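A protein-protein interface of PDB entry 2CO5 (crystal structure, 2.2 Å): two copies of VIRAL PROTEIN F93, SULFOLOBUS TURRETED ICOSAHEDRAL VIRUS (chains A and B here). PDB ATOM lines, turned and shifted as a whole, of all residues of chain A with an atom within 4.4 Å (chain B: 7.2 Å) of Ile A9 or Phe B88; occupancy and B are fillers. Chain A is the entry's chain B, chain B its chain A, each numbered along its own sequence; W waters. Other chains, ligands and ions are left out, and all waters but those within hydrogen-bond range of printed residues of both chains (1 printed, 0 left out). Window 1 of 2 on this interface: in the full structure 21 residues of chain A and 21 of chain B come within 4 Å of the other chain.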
ATOM      1  N   ARG A   8      26.438   4.974  12.408  1.00  0.00           N
ATOM      2  CA  ARG A   8      26.098   5.598  11.143  1.00  0.00           C
ATOM      3  C   ARG A   8      27.425   5.869  10.449  1.00  0.00           C
ATOM      4  O   ARG A   8      28.405   6.236  11.105  1.00  0.00           O
ATOM      5  CB  ARG A   8      25.346   6.907  11.380  1.00  0.00           C
ATOM      6  CG  ARG A   8      24.029   6.722  12.119  1.00  0.00           C
ATOM      7  CD  ARG A   8      23.459   8.054  12.574  1.00  0.00           C
ATOM      8  NE  ARG A   8      23.068   8.917  11.459  1.00  0.00           N
ATOM      9  CZ  ARG A   8      22.679  10.186  11.582  1.00  0.00           C
ATOM     10  NH1 ARG A   8      22.615  10.765  12.775  1.00  0.00           N
ATOM     11  NH2 ARG A   8      22.350  10.886  10.504  1.00  0.00           N
ATOM     12  N   ILE A   9      27.456   5.686   9.136  1.00  0.00           N
ATOM     13  CA  ILE A   9      28.690   5.745   8.377  1.00  0.00           C
ATOM     14  C   ILE A   9      29.369   7.121   8.496  1.00  0.00           C
ATOM     15  O   ILE A   9      30.587   7.205   8.550  1.00  0.00           O
ATOM     16  CB  ILE A   9      28.455   5.333   6.897  1.00  0.00           C
ATOM     17  CG1 ILE A   9      29.735   4.742   6.299  1.00  0.00           C
ATOM     18  CG2 ILE A   9      27.914   6.500   6.062  1.00  0.00           C
ATOM     19  CD1 ILE A   9      30.148   3.435   6.947  1.00  0.00           C
ATOM     20  N   ASN A  10      28.575   8.186   8.579  1.00  0.00           N
ATOM     21  CA  ASN A  10      29.131   9.532   8.629  1.00  0.00           C
ATOM     22  C   ASN A  10      29.852   9.815   9.946  1.00  0.00           C
ATOM     23  O   ASN A  10      30.854  10.533   9.960  1.00  0.00           O
ATOM     24  CB  ASN A  10      28.048  10.575   8.352  1.00  0.00           C
ATOM     25  CG  ASN A  10      27.737  10.717   6.868  1.00  0.00           C
ATOM     26  OD1 ASN A  10      26.788  11.405   6.480  1.00  0.00           O
ATOM     27  ND2 ASN A  10      28.549  10.090   6.033  1.00  0.00           N
ATOM     28  N   TYR A  11      29.354   9.238  11.043  1.00  0.00           N
ATOM     29  CA  TYR A  11      30.048   9.323  12.326  1.00  0.00           C
ATOM     30  C   TYR A  11      31.359   8.549  12.270  1.00  0.00           C
ATOM     31  O   TYR A  11      32.382   9.042  12.719  1.00  0.00           O
ATOM     32  CB  TYR A  11      29.188   8.790  13.477  1.00  0.00           C
ATOM     33  CG  TYR A  11      28.121   9.746  13.981  1.00  0.00           C
ATOM     34  CD1 TYR A  11      28.441  11.050  14.355  1.00  0.00           C
ATOM     35  CD2 TYR A  11      26.807   9.337  14.119  1.00  0.00           C
ATOM     36  CE1 TYR A  11      27.472  11.917  14.842  1.00  0.00           C
ATOM     37  CE2 TYR A  11      25.826  10.197  14.614  1.00  0.00           C
ATOM     38  CZ  TYR A  11      26.167  11.479  14.973  1.00  0.00           C
ATOM     39  OH  TYR A  11      25.206  12.339  15.439  1.00  0.00           O
ATOM     40  N   TYR A  12      31.321   7.338  11.721  1.00  0.00           N
ATOM     41  CA  TYR A  12      32.531   6.532  11.572  1.00  0.00           C
ATOM     42  C   TYR A  12      33.562   7.279  10.739  1.00  0.00           C
ATOM     43  O   TYR A  12      34.724   7.369  11.108  1.00  0.00           O
ATOM     44  CB  TYR A  12      32.224   5.181  10.924  1.00  0.00           C
ATOM     45  CG  TYR A  12      33.475   4.383  10.625  1.00  0.00           C
ATOM     46  CD1 TYR A  12      34.145   3.703  11.640  1.00  0.00           C
ATOM     47  CD2 TYR A  12      34.006   4.335   9.334  1.00  0.00           C
ATOM     48  CE1 TYR A  12      35.302   2.984  11.379  1.00  0.00           C
ATOM     49  CE2 TYR A  12      35.164   3.626   9.064  1.00  0.00           C
ATOM     50  CZ  TYR A  12      35.811   2.952  10.097  1.00  0.00           C
ATOM     51  OH  TYR A  12      36.952   2.236   9.848  1.00  0.00           O
ATOM     52  N   ILE A  13      33.118   7.828   9.620  1.00  0.00           N
ATOM     53  CA  ILE A  13      33.997   8.564   8.732  1.00  0.00           C
ATOM     54  C   ILE A  13      34.650   9.769   9.418  1.00  0.00           C
ATOM     55  O   ILE A  13      35.851   9.987   9.267  1.00  0.00           O
ATOM     56  CB  ILE A  13      33.242   9.008   7.469  1.00  0.00           C
ATOM     57  CG1 ILE A  13      33.021   7.805   6.556  1.00  0.00           C
ATOM     58  CG2 ILE A  13      34.010  10.085   6.748  1.00  0.00           C
ATOM     59  CD1 ILE A  13      32.006   8.039   5.477  1.00  0.00           C
ATOM     60  N   PHE A  88      31.442  -2.122  12.367  1.00  0.00           N
ATOM     61  CA  PHE A  88      31.336  -2.050  10.901  1.00  0.00           C
ATOM     62  C   PHE A  88      32.149  -3.132  10.197  1.00  0.00           C
ATOM     63  O   PHE A  88      31.720  -3.676   9.185  1.00  0.00           O
ATOM     64  CB  PHE A  88      31.732  -0.659  10.383  1.00  0.00           C
ATOM     65  CG  PHE A  88      30.617   0.359  10.466  1.00  0.00           C
ATOM     66  CD1 PHE A  88      30.683   1.419  11.356  1.00  0.00           C
ATOM     67  CD2 PHE A  88      29.501   0.246   9.654  1.00  0.00           C
ATOM     68  CE1 PHE A  88      29.663   2.341  11.438  1.00  0.00           C
ATOM     69  CE2 PHE A  88      28.472   1.168   9.731  1.00  0.00           C
ATOM     70  CZ  PHE A  88      28.555   2.220  10.633  1.00  0.00           C
ATOM     71  N   VAL A  92      30.181  -5.554   7.714  1.00  0.00           N
ATOM     72  CA  VAL A  92      30.458  -5.241   6.317  1.00  0.00           C
ATOM     73  C   VAL A  92      31.533  -6.122   5.684  1.00  0.00           C
ATOM     74  O   VAL A  92      31.366  -6.568   4.553  1.00  0.00           O
ATOM     75  CB  VAL A  92      30.854  -3.763   6.140  1.00  0.00           C
ATOM     76  CG1 VAL A  92      31.209  -3.473   4.677  1.00  0.00           C
ATOM     77  CG2 VAL A  92      29.712  -2.832   6.618  1.00  0.00           C
ATOM     78  N   ARG B   8      19.603   3.670   9.136  1.00  0.00           N
ATOM     79  CA  ARG B   8      19.810   2.933   7.876  1.00  0.00           C
ATOM     80  C   ARG B   8      20.577   1.636   8.082  1.00  0.00           C
ATOM     81  O   ARG B   8      20.381   0.674   7.343  1.00  0.00           O
ATOM     82  CB  ARG B   8      20.543   3.786   6.829  1.00  0.00           C
ATOM     83  CG  ARG B   8      20.970   3.008   5.561  1.00  0.00           C
ATOM     84  CD  ARG B   8      21.679   3.885   4.539  1.00  0.00           C
ATOM     85  NE  ARG B   8      22.967   4.365   5.039  1.00  0.00           N
ATOM     86  CZ  ARG B   8      23.747   5.247   4.421  1.00  0.00           C
ATOM     87  NH1 ARG B   8      23.385   5.777   3.256  1.00  0.00           N
ATOM     88  NH2 ARG B   8      24.892   5.613   4.979  1.00  0.00           N
ATOM     89  N   ILE B   9      21.455   1.598   9.075  1.00  0.00           N
ATOM     90  CA  ILE B   9      22.244   0.397   9.294  1.00  0.00           C
ATOM     91  C   ILE B   9      21.341  -0.840   9.458  1.00  0.00           C
ATOM     92  O   ILE B   9      21.744  -1.938   9.089  1.00  0.00           O
ATOM     93  CB  ILE B   9      23.239   0.564  10.486  1.00  0.00           C
ATOM     94  CG1 ILE B   9      24.296  -0.540  10.442  1.00  0.00           C
ATOM     95  CG2 ILE B   9      22.513   0.588  11.818  1.00  0.00           C
ATOM     96  CD1 ILE B   9      24.987  -0.647   9.083  1.00  0.00           C
ATOM     97  N   TYR B  12      20.562  -2.262   6.038  1.00  0.00           N
ATOM     98  CA  TYR B  12      21.709  -3.007   5.520  1.00  0.00           C
ATOM     99  C   TYR B  12      21.803  -4.413   6.139  1.00  0.00           C
ATOM    100  O   TYR B  12      22.045  -5.395   5.428  1.00  0.00           O
ATOM    101  CB  TYR B  12      23.025  -2.229   5.738  1.00  0.00           C
ATOM    102  CG  TYR B  12      24.232  -3.029   5.304  1.00  0.00           C
ATOM    103  CD1 TYR B  12      24.618  -3.077   3.968  1.00  0.00           C
ATOM    104  CD2 TYR B  12      24.955  -3.783   6.221  1.00  0.00           C
ATOM    105  CE1 TYR B  12      25.707  -3.837   3.560  1.00  0.00           C
ATOM    106  CE2 TYR B  12      26.046  -4.543   5.824  1.00  0.00           C
ATOM    107  CZ  TYR B  12      26.412  -4.571   4.495  1.00  0.00           C
ATOM    108  OH  TYR B  12      27.485  -5.332   4.110  1.00  0.00           O
ATOM    109  N   ILE B  13      21.612  -4.495   7.457  1.00  0.00           N
ATOM    110  CA  ILE B  13      21.719  -5.758   8.187  1.00  0.00           C
ATOM    111  C   ILE B  13      20.633  -6.730   7.733  1.00  0.00           C
ATOM    112  O   ILE B  13      20.902  -7.911   7.542  1.00  0.00           O
ATOM    113  CB  ILE B  13      21.648  -5.531   9.724  1.00  0.00           C
ATOM    114  CG1 ILE B  13      22.925  -4.847  10.221  1.00  0.00           C
ATOM    115  CG2 ILE B  13      21.478  -6.840  10.497  1.00  0.00           C
ATOM    116  CD1 ILE B  13      22.845  -4.378  11.653  1.00  0.00           C
ATOM    117  N   GLU B  82      23.851  -4.738  -3.144  1.00  0.00           N
ATOM    118  CA  GLU B  82      25.182  -4.713  -3.735  1.00  0.00           C
ATOM    119  C   GLU B  82      25.742  -3.291  -3.728  1.00  0.00           C
ATOM    120  O   GLU B  82      26.876  -3.081  -3.317  1.00  0.00           O
ATOM    121  CB  GLU B  82      25.176  -5.286  -5.160  1.00  0.00           C
ATOM    122  CG  GLU B  82      24.868  -6.784  -5.261  1.00  0.00           C
ATOM    123  CD  GLU B  82      25.876  -7.675  -4.546  1.00  0.00           C
ATOM    124  OE1 GLU B  82      27.028  -7.239  -4.324  1.00  0.00           O
ATOM    125  OE2 GLU B  82      25.511  -8.823  -4.209  1.00  0.00           O
ATOM    126  N   GLU B  83      24.938  -2.320  -4.160  1.00  0.00           N
ATOM    127  CA  GLU B  83      25.373  -0.916  -4.202  1.00  0.00           C
ATOM    128  C   GLU B  83      25.792  -0.425  -2.816  1.00  0.00           C
ATOM    129  O   GLU B  83      26.852   0.177  -2.646  1.00  0.00           O
ATOM    130  CB  GLU B  83      24.253  -0.010  -4.731  1.00  0.00           C
ATOM    131  CG  GLU B  83      24.014  -0.096  -6.231  1.00  0.00           C
ATOM    132  CD  GLU B  83      22.772   0.665  -6.686  1.00  0.00           C
ATOM    133  OE1 GLU B  83      21.767   0.696  -5.942  1.00  0.00           O
ATOM    134  OE2 GLU B  83      22.801   1.225  -7.801  1.00  0.00           O
ATOM    135  N   LEU B  84      24.946  -0.687  -1.833  1.00  0.00           N
ATOM    136  CA  LEU B  84      25.204  -0.231  -0.471  1.00  0.00           C
ATOM    137  C   LEU B  84      26.395  -0.975   0.132  1.00  0.00           C
ATOM    138  O   LEU B  84      27.222  -0.387   0.820  1.00  0.00           O
ATOM    139  CB  LEU B  84      23.949  -0.409   0.395  1.00  0.00           C
ATOM    140  CG  LEU B  84      23.902   0.359   1.719  1.00  0.00           C
ATOM    141  CD1 LEU B  84      24.328   1.820   1.568  1.00  0.00           C
ATOM    142  CD2 LEU B  84      22.498   0.259   2.316  1.00  0.00           C
ATOM    143  N   HIS B  85      26.476  -2.273  -0.142  1.00  0.00           N
ATOM    144  CA  HIS B  85      27.604  -3.076   0.292  1.00  0.00           C
ATOM    145  C   HIS B  85      28.919  -2.542  -0.280  1.00  0.00           C
ATOM    146  O   HIS B  85      29.873  -2.331   0.464  1.00  0.00           O
ATOM    147  CB  HIS B  85      27.408  -4.532  -0.103  1.00  0.00           C
ATOM    148  CG  HIS B  85      28.554  -5.408   0.279  1.00  0.00           C
ATOM    149  ND1 HIS B  85      29.022  -5.492   1.572  1.00  0.00           N
ATOM    150  CD2 HIS B  85      29.331  -6.234  -0.460  1.00  0.00           C
ATOM    151  CE1 HIS B  85      30.041  -6.332   1.612  1.00  0.00           C
ATOM    152  NE2 HIS B  85      30.247  -6.798   0.394  1.00  0.00           N
ATOM    153  N   GLU B  86      28.969  -2.310  -1.590  1.00  0.00           N
ATOM    154  CA  GLU B  86      30.181  -1.750  -2.202  1.00  0.00           C
ATOM    155  C   GLU B  86      30.532  -0.406  -1.574  1.00  0.00           C
ATOM    156  O   GLU B  86      31.706  -0.113  -1.332  1.00  0.00           O
ATOM    157  CB  GLU B  86      30.032  -1.579  -3.721  1.00  0.00           C
ATOM    158  CG  GLU B  86      29.812  -2.872  -4.508  1.00  0.00           C
ATOM    159  CD  GLU B  86      30.989  -3.837  -4.470  1.00  0.00           C
ATOM    160  OE1 GLU B  86      32.126  -3.416  -4.160  1.00  0.00           O
ATOM    161  OE2 GLU B  86      30.765  -5.033  -4.764  1.00  0.00           O
ATOM    162  N   PHE B  87      29.515   0.408  -1.312  1.00  0.00           N
ATOM    163  CA  PHE B  87      29.727   1.716  -0.713  1.00  0.00           C
ATOM    164  C   PHE B  87      30.356   1.572   0.686  1.00  0.00           C
ATOM    165  O   PHE B  87      31.407   2.142   0.946  1.00  0.00           O
ATOM    166  CB  PHE B  87      28.412   2.504  -0.688  1.00  0.00           C
ATOM    167  CG  PHE B  87      28.490   3.815   0.051  1.00  0.00           C
ATOM    168  CD1 PHE B  87      29.152   4.902  -0.501  1.00  0.00           C
ATOM    169  CD2 PHE B  87      27.876   3.965   1.289  1.00  0.00           C
ATOM    170  CE1 PHE B  87      29.215   6.111   0.172  1.00  0.00           C
ATOM    171  CE2 PHE B  87      27.933   5.173   1.965  1.00  0.00           C
ATOM    172  CZ  PHE B  87      28.605   6.247   1.405  1.00  0.00           C
ATOM    173  N   PHE B  88      29.738   0.794   1.573  1.00  0.00           N
ATOM    174  CA  PHE B  88      30.302   0.574   2.918  1.00  0.00           C
ATOM    175  C   PHE B  88      31.676  -0.113   2.915  1.00  0.00           C
ATOM    176  O   PHE B  88      32.546   0.222   3.713  1.00  0.00           O
ATOM    177  CB  PHE B  88      29.358  -0.271   3.779  1.00  0.00           C
ATOM    178  CG  PHE B  88      28.101   0.437   4.215  1.00  0.00           C
ATOM    179  CD1 PHE B  88      27.974   1.819   4.148  1.00  0.00           C
ATOM    180  CD2 PHE B  88      27.046  -0.298   4.730  1.00  0.00           C
ATOM    181  CE1 PHE B  88      26.820   2.435   4.557  1.00  0.00           C
ATOM    182  CE2 PHE B  88      25.891   0.321   5.141  1.00  0.00           C
ATOM    183  CZ  PHE B  88      25.780   1.687   5.059  1.00  0.00           C
ATOM    184  N   LYS B  89      31.856  -1.079   2.026  1.00  0.00           N
ATOM    185  CA  LYS B  89      33.075  -1.882   1.989  1.00  0.00           C
ATOM    186  C   LYS B  89      34.330  -1.055   1.722  1.00  0.00           C
ATOM    187  O   LYS B  89      35.384  -1.288   2.332  1.00  0.00           O
ATOM    188  CB  LYS B  89      32.937  -2.989   0.938  1.00  0.00           C
ATOM    189  CG  LYS B  89      34.025  -4.035   0.977  1.00  0.00           C
ATOM    190  CD  LYS B  89      33.654  -5.270   0.140  1.00  0.00           C
ATOM    191  CE  LYS B  89      33.831  -5.042  -1.365  1.00  0.00           C
ATOM    192  NZ  LYS B  89      35.254  -5.129  -1.803  1.00  0.00           N
ATOM    193  N   LYS B  90      34.213  -0.091   0.812  1.00  0.00           N
ATOM    194  CA  LYS B  90      35.345   0.753   0.445  1.00  0.00           C
ATOM    195  C   LYS B  90      35.705   1.704   1.592  1.00  0.00           C
ATOM    196  O   LYS B  90      36.875   2.003   1.801  1.00  0.00           O
ATOM    197  CB  LYS B  90      35.087   1.458  -0.908  1.00  0.00           C
ATOM    198  CG  LYS B  90      35.236   2.977  -0.953  1.00  0.00           C
ATOM    199  CD  LYS B  90      33.928   3.665  -0.557  1.00  0.00           C
ATOM    200  CE  LYS B  90      34.045   5.175  -0.597  1.00  0.00           C
ATOM    201  NZ  LYS B  90      35.193   5.644   0.210  1.00  0.00           N
ATOM    202  N   ILE B  91      34.694   2.147   2.340  1.00  0.00           N
ATOM    203  CA  ILE B  91      34.900   3.016   3.498  1.00  0.00           C
ATOM    204  C   ILE B  91      35.538   2.234   4.652  1.00  0.00           C
ATOM    205  O   ILE B  91      36.550   2.646   5.212  1.00  0.00           O
ATOM    206  CB  ILE B  91      33.562   3.621   4.007  1.00  0.00           C
ATOM    207  CG1 ILE B  91      32.922   4.520   2.941  1.00  0.00           C
ATOM    208  CG2 ILE B  91      33.779   4.401   5.303  1.00  0.00           C
ATOM    209  CD1 ILE B  91      31.502   4.958   3.266  1.00  0.00           C
ATOM    210  N   VAL B  92      34.947   1.093   4.979  1.00  0.00           N
ATOM    211  CA  VAL B  92      35.243   0.385   6.223  1.00  0.00           C
ATOM    212  C   VAL B  92      36.382  -0.625   6.099  1.00  0.00           C
ATOM    213  O   VAL B  92      37.240  -0.706   6.985  1.00  0.00           O
ATOM    214  CB  VAL B  92      33.988  -0.339   6.733  1.00  0.00           C
ATOM    215  CG1 VAL B  92      34.316  -1.237   7.929  1.00  0.00           C
ATOM    216  CG2 VAL B  92      32.911   0.688   7.086  1.00  0.00           C
ATOM    217  N   CYS B  93      36.391  -1.388   5.009  1.00  0.00           N
ATOM    218  CA  CYS B  93      37.261  -2.550   4.912  1.00  0.00           C
ATOM    219  C   CYS B  93      38.589  -2.210   4.244  1.00  0.00           C
ATOM    220  O   CYS B  93      38.619  -1.826   3.075  1.00  0.00           O
ATOM    221  CB  CYS B  93      36.561  -3.683   4.163  1.00  0.00           C
ATOM    222  SG  CYS B  93      34.900  -4.071   4.761  1.00  0.00           S
HETATM  223  O   HOH W   1      38.269   2.598   7.299  1.00  0.00           O
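Of the 8 printed residues of chain A, 4 touch a printed residue of chain B.
Printed residues of chain A that touch a printed residue of chain B: Ile A9, Ile A13, Phe A88 and Val A92.
Hydrophobic or aromatic side chains of chain A within 4 Å of the printed part of chain B: Ile A9, Ile A13, Phe A88 and Val A92.
Along chain B the printed residues that touch a printed residue of chain A span positions 8 to 93.
Among the printed residues, 12 pairs touch across the chains.
Among the printed residues, no Asp or Glu carboxylate lies within 4 Å of a Lys or Arg side-chain nitrogen of the other chain.
Among the printed residues, pairs that only touch across the chains: Ile A9 with Arg B8 (3.3 Å), Ile A9 with Phe B88 (3.9 Å), Ile A9 with Ile B91 (3.5 Å), Ile A9 with Val B92 (3.9 Å), Ile A13 with Ile B91 (3.7 Å), Phe A88 with Ile B9 (3.98 Å), Phe A88 with Val B92 (3.6 Å), Val A92 with Tyr B12 (3.7 Å), Val A92 with His B85 (3.2 Å), Val A92 with Phe B88 (3.8 Å), Val A92 with Lys B89 (3.6 Å) and Val A92 with Cys B93 (3.7 Å).
Water W1 lies within hydrogen-bond range of O of Ile B91 (2.7 Å), OH of Tyr A12 (2.9 Å) and O of Val B92 (3.5 Å).
Of the printed residues of chain B, Ile A9 touches Arg B8, Phe B88, Ile B91 and Val B92.
Of chain A, only Ile A9 and Val A92 come within 4 Å of Phe B88.
Of the printed residues of chain B, Val A92 touches Tyr B12 (3.7 Å), His B85 (3.2 Å), Phe B88 (3.8 Å), Lys B89 (3.6 Å) and Cys B93 (3.7 Å).
Printed residues of chain A within 4 Å of His B85: Val A92 (3.2 Å).
Of the printed residues of chain A, Ile B91 touches Ile A9 (3.5 Å) and Ile A13 (3.7 Å).
Printed residues of chain A within 4 Å of Val B92: Ile A9 (3.9 Å) and Phe A88 (3.6 Å).
Of the printed residues of chain A, Cys B93 touches Val A92 (3.7 Å).
Arg A8 touches none of the printed residues of chain B.
Tyr A12 touches none of the printed residues of chain B.
The nearest printed residue of chain A that does not touch Phe B88 is Phe A88 (5.3 Å).
The side-chain hydroxyl of Tyr B12 lies within hydrogen-bond range of a ring nitrogen (ND1) of His B85 (3.0 Å).
Ile A9 touches Arg B8, but with the chains exchanged Arg A8 does not touch Ile B9 (5.8 Å).
Ile A9 touches Phe B88, and with the chains exchanged Phe A88 touches Ile B9.
Ile A9 touches Val B92, but with the chains exchanged Val A92 does not touch Ile B9 (5.8 Å).
Phe A88 touches Val B92, and with the chains exchanged Val A92 touches Phe B88.
Positions printed for both chains: 8, 9, 12, 13, 88 and 92.
Of the 12 pairs that touch across the chains among the printed residues, 4 have their exchanged pair printed and touching as well.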
